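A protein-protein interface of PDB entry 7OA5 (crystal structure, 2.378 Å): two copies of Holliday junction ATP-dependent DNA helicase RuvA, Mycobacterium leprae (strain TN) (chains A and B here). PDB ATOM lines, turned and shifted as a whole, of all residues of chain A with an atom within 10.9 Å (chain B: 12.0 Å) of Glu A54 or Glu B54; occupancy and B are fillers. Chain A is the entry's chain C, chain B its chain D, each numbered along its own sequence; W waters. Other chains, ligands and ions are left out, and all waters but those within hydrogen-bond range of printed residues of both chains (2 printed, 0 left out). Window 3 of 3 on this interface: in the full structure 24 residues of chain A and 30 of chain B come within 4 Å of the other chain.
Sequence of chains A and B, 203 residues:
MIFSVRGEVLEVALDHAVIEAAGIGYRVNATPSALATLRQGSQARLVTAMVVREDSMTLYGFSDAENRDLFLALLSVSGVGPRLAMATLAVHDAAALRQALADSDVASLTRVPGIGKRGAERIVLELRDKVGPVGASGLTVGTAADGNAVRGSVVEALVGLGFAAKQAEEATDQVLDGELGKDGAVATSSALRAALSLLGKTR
Glu A54 touches Val B52, but with the chains exchanged Val A52 does not touch Glu B54 (9.5 Å).
Glu A54 touches Arg B53, but with the chains exchanged Arg A53 does not touch Glu B54 (6.8 Å).
Glu B54 touches its own counterpart, Glu A54.
Asp A55 touches Val B52, but with the chains exchanged Val A52 does not touch Asp B55 (11.1 Å).
NH1 of Arg B53 lies within salt-bridge range of OD1 of Asp A55 (3.9 Å).
The backbone carbonyl oxygen (O) of Val B52 sits close to the backbone carbonyl oxygen (O) of Asp A55, at 3.4 Å.
O of Glu A54 touches CG1 of Val B52, 3.6 Å away.
Arg B53 touches Glu A54 (C to O, 3.5 Å).
N of Glu B54 touches O of Glu A54, at 3.6 Å.
Ser A56 touches Val B52.
O of Met A57 touches CB of Met B1, at 3.3 Å.
CB of Met A57 touches CE of Met B50 (3.8 Å).
Of chain A, only Glu A54 comes within 4 Å of Glu B54.
Asp A55 touches two residues of chain B.
Of chain B, only Val B52 comes within 4 Å of Ser A56.
Of chain A, only Glu A54, Asp A55 and Ser A56 come within 4 Å of Val B52.
No residue of chain A comes within 4 Å of Asp B55.
Of the printed residues of chain A, Met B1 touches Met A57 (3.3 Å).
Of the printed residues of chain B, Met A57 touches Met B1 (3.3 Å) and Met B50 (3.8 Å).
Pro B82 touches none of the printed residues of chain A.
The nearest residue of chain A that does not touch Glu B54 is Asp A55 (4.1 Å).
Water W1 lies within hydrogen-bond range of the side-chain carboxylate of Asp A55 (2.8 Å), the backbone NH of Glu B54 (3.0 Å) and the side-chain carboxylate of Glu A54 (3.1 Å).
Water W2 lies within hydrogen-bond range of O of Asp A55 and N of Val B52.
Of the 8 printed residues of chain A, 4 touch a printed residue of chain B.
Printed residues of chain A that touch a printed residue of chain B: Glu A54, Asp A55, Ser A56 and Met A57.
Among the printed residues, 8 pairs touch across the chains.
Among the printed residues, Asp or Glu carboxylates within 4 Å of a Lys or Arg side-chain nitrogen of the other chain: Asp A55 with Arg B53.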
ATOM      1  N   VAL A  51      -4.166   2.356  30.490  1.00  0.00           N
ATOM      2  CA  VAL A  51      -5.506   1.820  30.586  1.00  0.00           C
ATOM      3  C   VAL A  51      -5.424   0.322  30.380  1.00  0.00           C
ATOM      4  O   VAL A  51      -4.928  -0.158  29.361  1.00  0.00           O
ATOM      5  CB  VAL A  51      -6.496   2.517  29.625  1.00  0.00           C
ATOM      6  CG1 VAL A  51      -7.858   1.831  29.656  1.00  0.00           C
ATOM      7  CG2 VAL A  51      -6.632   4.000  29.983  1.00  0.00           C
ATOM      8  N   VAL A  52      -5.831  -0.414  31.401  1.00  0.00           N
ATOM      9  CA  VAL A  52      -5.782  -1.855  31.412  1.00  0.00           C
ATOM     10  C   VAL A  52      -7.190  -2.395  31.251  1.00  0.00           C
ATOM     11  O   VAL A  52      -8.110  -1.929  31.901  1.00  0.00           O
ATOM     12  CB  VAL A  52      -5.127  -2.340  32.741  1.00  0.00           C
ATOM     13  CG1 VAL A  52      -5.271  -3.844  32.924  1.00  0.00           C
ATOM     14  CG2 VAL A  52      -3.671  -1.925  32.800  1.00  0.00           C
ATOM     15  N   ARG A  53      -7.374  -3.312  30.330  1.00  0.00           N
ATOM     16  CA  ARG A  53      -8.650  -3.996  30.078  1.00  0.00           C
ATOM     17  C   ARG A  53      -8.316  -5.483  29.899  1.00  0.00           C
ATOM     18  O   ARG A  53      -7.144  -5.831  29.718  1.00  0.00           O
ATOM     19  CB  ARG A  53      -9.356  -3.450  28.823  1.00  0.00           C
ATOM     20  CG  ARG A  53      -9.772  -1.991  28.902  1.00  0.00           C
ATOM     21  CD  ARG A  53     -10.803  -1.738  29.988  1.00  0.00           C
ATOM     22  NE  ARG A  53     -11.107  -0.310  30.137  1.00  0.00           N
ATOM     23  CZ  ARG A  53     -10.729   0.439  31.173  1.00  0.00           C
ATOM     24  NH1 ARG A  53     -10.046  -0.099  32.176  1.00  0.00           N
ATOM     25  NH2 ARG A  53     -11.039   1.730  31.216  1.00  0.00           N
ATOM     26  N   GLU A  54      -9.314  -6.369  29.918  1.00  0.00           N
ATOM     27  CA  GLU A  54      -9.076  -7.814  29.765  1.00  0.00           C
ATOM     28  C   GLU A  54      -8.195  -8.175  28.562  1.00  0.00           C
ATOM     29  O   GLU A  54      -7.289  -9.003  28.692  1.00  0.00           O
ATOM     30  CB  GLU A  54     -10.412  -8.572  29.698  1.00  0.00           C
ATOM     31  CG  GLU A  54     -10.270 -10.073  29.510  1.00  0.00           C
ATOM     32  CD  GLU A  54     -11.573 -10.819  29.307  1.00  0.00           C
ATOM     33  OE1 GLU A  54     -12.640 -10.256  29.641  1.00  0.00           O
ATOM     34  OE2 GLU A  54     -11.526 -11.976  28.827  1.00  0.00           O
ATOM     35  N   ASP A  55      -8.452  -7.551  27.408  1.00  0.00           N
ATOM     36  CA  ASP A  55      -7.727  -7.849  26.187  1.00  0.00           C
ATOM     37  C   ASP A  55      -6.853  -6.704  25.693  1.00  0.00           C
ATOM     38  O   ASP A  55      -6.509  -6.695  24.511  1.00  0.00           O
ATOM     39  CB  ASP A  55      -8.711  -8.222  25.059  1.00  0.00           C
ATOM     40  CG  ASP A  55      -9.359  -9.584  25.175  1.00  0.00           C
ATOM     41  OD1 ASP A  55      -8.818 -10.448  25.916  1.00  0.00           O
ATOM     42  OD2 ASP A  55     -10.410  -9.795  24.525  1.00  0.00           O
ATOM     43  N   SER A  56      -6.484  -5.745  26.569  1.00  0.00           N
ATOM     44  CA  SER A  56      -5.626  -4.649  26.133  1.00  0.00           C
ATOM     45  C   SER A  56      -4.882  -3.963  27.246  1.00  0.00           C
ATOM     46  O   SER A  56      -5.312  -3.937  28.391  1.00  0.00           O
ATOM     47  CB  SER A  56      -6.398  -3.628  25.293  1.00  0.00           C
ATOM     48  OG  SER A  56      -7.375  -2.944  26.058  1.00  0.00           O
ATOM     49  N   MET A  57      -3.728  -3.423  26.891  1.00  0.00           N
ATOM     50  CA  MET A  57      -2.904  -2.594  27.742  1.00  0.00           C
ATOM     51  C   MET A  57      -2.491  -1.459  26.835  1.00  0.00           C
ATOM     52  O   MET A  57      -1.865  -1.695  25.810  1.00  0.00           O
ATOM     53  CB  MET A  57      -1.716  -3.367  28.280  1.00  0.00           C
ATOM     54  CG  MET A  57      -2.053  -4.060  29.548  1.00  0.00           C
ATOM     55  SD  MET A  57      -0.629  -4.766  30.373  1.00  0.00           S
ATOM     56  CE  MET A  57       0.440  -3.351  30.494  1.00  0.00           C
ATOM     57  N   THR A  58      -2.932  -0.257  27.141  1.00  0.00           N
ATOM     58  CA  THR A  58      -2.703   0.884  26.253  1.00  0.00           C
ATOM     59  C   THR A  58      -2.211   2.084  27.027  1.00  0.00           C
ATOM     60  O   THR A  58      -2.679   2.329  28.124  1.00  0.00           O
ATOM     61  CB  THR A  58      -4.007   1.249  25.508  1.00  0.00           C
ATOM     62  OG1 THR A  58      -4.688   0.068  25.084  1.00  0.00           O
ATOM     63  CG2 THR A  58      -3.766   2.145  24.306  1.00  0.00           C
ATOM     64  N   MET B   1       0.901  -2.495  23.558  1.00  0.00           N
ATOM     65  CA  MET B   1       1.628  -1.390  24.174  1.00  0.00           C
ATOM     66  C   MET B   1       3.081  -1.436  23.757  1.00  0.00           C
ATOM     67  O   MET B   1       3.676  -0.411  23.519  1.00  0.00           O
ATOM     68  CB  MET B   1       1.463  -1.487  25.691  1.00  0.00           C
ATOM     69  CG  MET B   1       2.304  -0.559  26.481  1.00  0.00           C
ATOM     70  SD  MET B   1       1.771  -0.760  28.165  1.00  0.00           S
ATOM     71  CE  MET B   1       3.194  -1.470  28.888  1.00  0.00           C
ATOM     72  N   MET B  50       1.982  -6.681  20.971  1.00  0.00           N
ATOM     73  CA  MET B  50       1.720  -7.377  22.229  1.00  0.00           C
ATOM     74  C   MET B  50       0.259  -7.762  22.227  1.00  0.00           C
ATOM     75  O   MET B  50      -0.609  -6.911  22.014  1.00  0.00           O
ATOM     76  CB  MET B  50       2.038  -6.495  23.444  1.00  0.00           C
ATOM     77  CG  MET B  50       1.889  -7.212  24.752  1.00  0.00           C
ATOM     78  SD  MET B  50       2.348  -6.209  26.212  1.00  0.00           S
ATOM     79  CE  MET B  50       0.981  -5.116  26.280  1.00  0.00           C
ATOM     80  N   VAL B  51      -0.018  -9.052  22.389  1.00  0.00           N
ATOM     81  CA  VAL B  51      -1.386  -9.538  22.433  1.00  0.00           C
ATOM     82  C   VAL B  51      -1.693  -9.886  23.868  1.00  0.00           C
ATOM     83  O   VAL B  51      -0.993 -10.687  24.498  1.00  0.00           O
ATOM     84  CB  VAL B  51      -1.648 -10.690  21.444  1.00  0.00           C
ATOM     85  CG1 VAL B  51      -3.027 -11.275  21.643  1.00  0.00           C
ATOM     86  CG2 VAL B  51      -1.481 -10.203  20.014  1.00  0.00           C
ATOM     87  N   VAL B  52      -2.680  -9.186  24.422  1.00  0.00           N
ATOM     88  CA  VAL B  52      -3.101  -9.339  25.801  1.00  0.00           C
ATOM     89  C   VAL B  52      -4.399 -10.091  25.834  1.00  0.00           C
ATOM     90  O   VAL B  52      -5.307  -9.786  25.074  1.00  0.00           O
ATOM     91  CB  VAL B  52      -3.227  -7.940  26.468  1.00  0.00           C
ATOM     92  CG1 VAL B  52      -3.901  -8.013  27.825  1.00  0.00           C
ATOM     93  CG2 VAL B  52      -1.866  -7.287  26.593  1.00  0.00           C
ATOM     94  N   ARG B  53      -4.457 -11.132  26.643  1.00  0.00           N
ATOM     95  CA  ARG B  53      -5.660 -11.925  26.876  1.00  0.00           C
ATOM     96  C   ARG B  53      -5.765 -12.116  28.395  1.00  0.00           C
ATOM     97  O   ARG B  53      -4.805 -11.861  29.128  1.00  0.00           O
ATOM     98  CB  ARG B  53      -5.603 -13.286  26.151  1.00  0.00           C
ATOM     99  CG  ARG B  53      -5.534 -13.190  24.631  1.00  0.00           C
ATOM    100  CD  ARG B  53      -6.789 -12.573  24.045  1.00  0.00           C
ATOM    101  NE  ARG B  53      -6.669 -12.367  22.600  1.00  0.00           N
ATOM    102  CZ  ARG B  53      -6.575 -11.178  22.010  1.00  0.00           C
ATOM    103  NH1 ARG B  53      -6.593 -10.064  22.732  1.00  0.00           N
ATOM    104  NH2 ARG B  53      -6.458 -11.094  20.689  1.00  0.00           N
ATOM    105  N   GLU B  54      -6.922 -12.568  28.887  1.00  0.00           N
ATOM    106  CA  GLU B  54      -7.130 -12.781  30.326  1.00  0.00           C
ATOM    107  C   GLU B  54      -6.011 -13.609  30.995  1.00  0.00           C
ATOM    108  O   GLU B  54      -5.557 -13.270  32.074  1.00  0.00           O
ATOM    109  CB  GLU B  54      -8.496 -13.442  30.575  1.00  0.00           C
ATOM    110  CG  GLU B  54      -8.782 -13.626  32.059  1.00  0.00           C
ATOM    111  CD  GLU B  54     -10.076 -14.323  32.423  1.00  0.00           C
ATOM    112  OE1 GLU B  54     -10.091 -15.030  33.455  1.00  0.00           O
ATOM    113  OE2 GLU B  54     -11.080 -14.154  31.691  1.00  0.00           O
ATOM    114  N   ASP B  55      -5.559 -14.653  30.332  1.00  0.00           N
ATOM    115  CA  ASP B  55      -4.547 -15.555  30.853  1.00  0.00           C
ATOM    116  C   ASP B  55      -3.238 -15.571  30.068  1.00  0.00           C
ATOM    117  O   ASP B  55      -2.489 -16.535  30.182  1.00  0.00           O
ATOM    118  CB  ASP B  55      -5.113 -16.979  30.982  1.00  0.00           C
ATOM    119  CG  ASP B  55      -5.975 -17.447  29.811  1.00  0.00           C
ATOM    120  OD1 ASP B  55      -5.943 -16.775  28.719  1.00  0.00           O
ATOM    121  OD2 ASP B  55      -6.696 -18.474  29.976  1.00  0.00           O
ATOM    122  N   SER B  56      -2.936 -14.510  29.305  1.00  0.00           N
ATOM    123  CA  SER B  56      -1.684 -14.469  28.554  1.00  0.00           C
ATOM    124  C   SER B  56      -1.258 -13.085  28.114  1.00  0.00           C
ATOM    125  O   SER B  56      -2.077 -12.197  27.918  1.00  0.00           O
ATOM    126  CB  SER B  56      -1.707 -15.418  27.350  1.00  0.00           C
ATOM    127  OG  SER B  56      -2.619 -14.997  26.353  1.00  0.00           O
ATOM    128  N   MET B  57       0.042 -12.914  27.967  1.00  0.00           N
ATOM    129  CA  MET B  57       0.658 -11.717  27.438  1.00  0.00           C
ATOM    130  C   MET B  57       1.736 -12.239  26.509  1.00  0.00           C
ATOM    131  O   MET B  57       2.642 -12.930  26.951  1.00  0.00           O
ATOM    132  CB  MET B  57       1.227 -10.850  28.552  1.00  0.00           C
ATOM    133  CG  MET B  57       0.198  -9.922  29.111  1.00  0.00           C
ATOM    134  SD  MET B  57       0.852  -8.762  30.298  1.00  0.00           S
ATOM    135  CE  MET B  57       2.156  -8.060  29.383  1.00  0.00           C
ATOM    136  N   THR B  58       1.579 -11.998  25.210  1.00  0.00           N
ATOM    137  CA  THR B  58       2.479 -12.569  24.215  1.00  0.00           C
ATOM    138  C   THR B  58       2.996 -11.516  23.256  1.00  0.00           C
ATOM    139  O   THR B  58       2.239 -10.650  22.857  1.00  0.00           O
ATOM    140  CB  THR B  58       1.760 -13.680  23.435  1.00  0.00           C
ATOM    141  OG1 THR B  58       0.997 -14.495  24.325  1.00  0.00           O
ATOM    142  CG2 THR B  58       2.717 -14.557  22.653  1.00  0.00           C
ATOM    143  N   TYR B  60       4.680 -10.737  19.510  1.00  0.00           N
ATOM    144  CA  TYR B  60       4.856 -11.237  18.154  1.00  0.00           C
ATOM    145  C   TYR B  60       5.821 -10.285  17.460  1.00  0.00           C
ATOM    146  O   TYR B  60       5.688  -9.088  17.599  1.00  0.00           O
ATOM    147  CB  TYR B  60       3.515 -11.381  17.430  1.00  0.00           C
ATOM    148  CG  TYR B  60       2.640 -12.396  18.133  1.00  0.00           C
ATOM    149  CD1 TYR B  60       2.756 -13.751  17.861  1.00  0.00           C
ATOM    150  CD2 TYR B  60       1.743 -12.005  19.119  1.00  0.00           C
ATOM    151  CE1 TYR B  60       1.964 -14.685  18.517  1.00  0.00           C
ATOM    152  CE2 TYR B  60       0.962 -12.933  19.794  1.00  0.00           C
ATOM    153  CZ  TYR B  60       1.066 -14.269  19.482  1.00  0.00           C
ATOM    154  OH  TYR B  60       0.269 -15.166  20.149  1.00  0.00           O
ATOM    155  N   PRO B  82      -3.798 -15.068  16.548  1.00  0.00           N
ATOM    156  CA  PRO B  82      -2.353 -14.853  16.411  1.00  0.00           C
ATOM    157  C   PRO B  82      -1.602 -15.936  15.650  1.00  0.00           C
ATOM    158  O   PRO B  82      -0.752 -15.600  14.845  1.00  0.00           O
ATOM    159  CB  PRO B  82      -1.898 -14.717  17.859  1.00  0.00           C
ATOM    160  CG  PRO B  82      -3.106 -14.186  18.583  1.00  0.00           C
ATOM    161  CD  PRO B  82      -4.222 -14.983  17.958  1.00  0.00           C
HETATM  162  O   HOH W   1      -9.236 -12.938  27.048  1.00  0.00           O
HETATM  163  O   HOH W   2      -4.117  -6.911  22.990  1.00  0.00           O
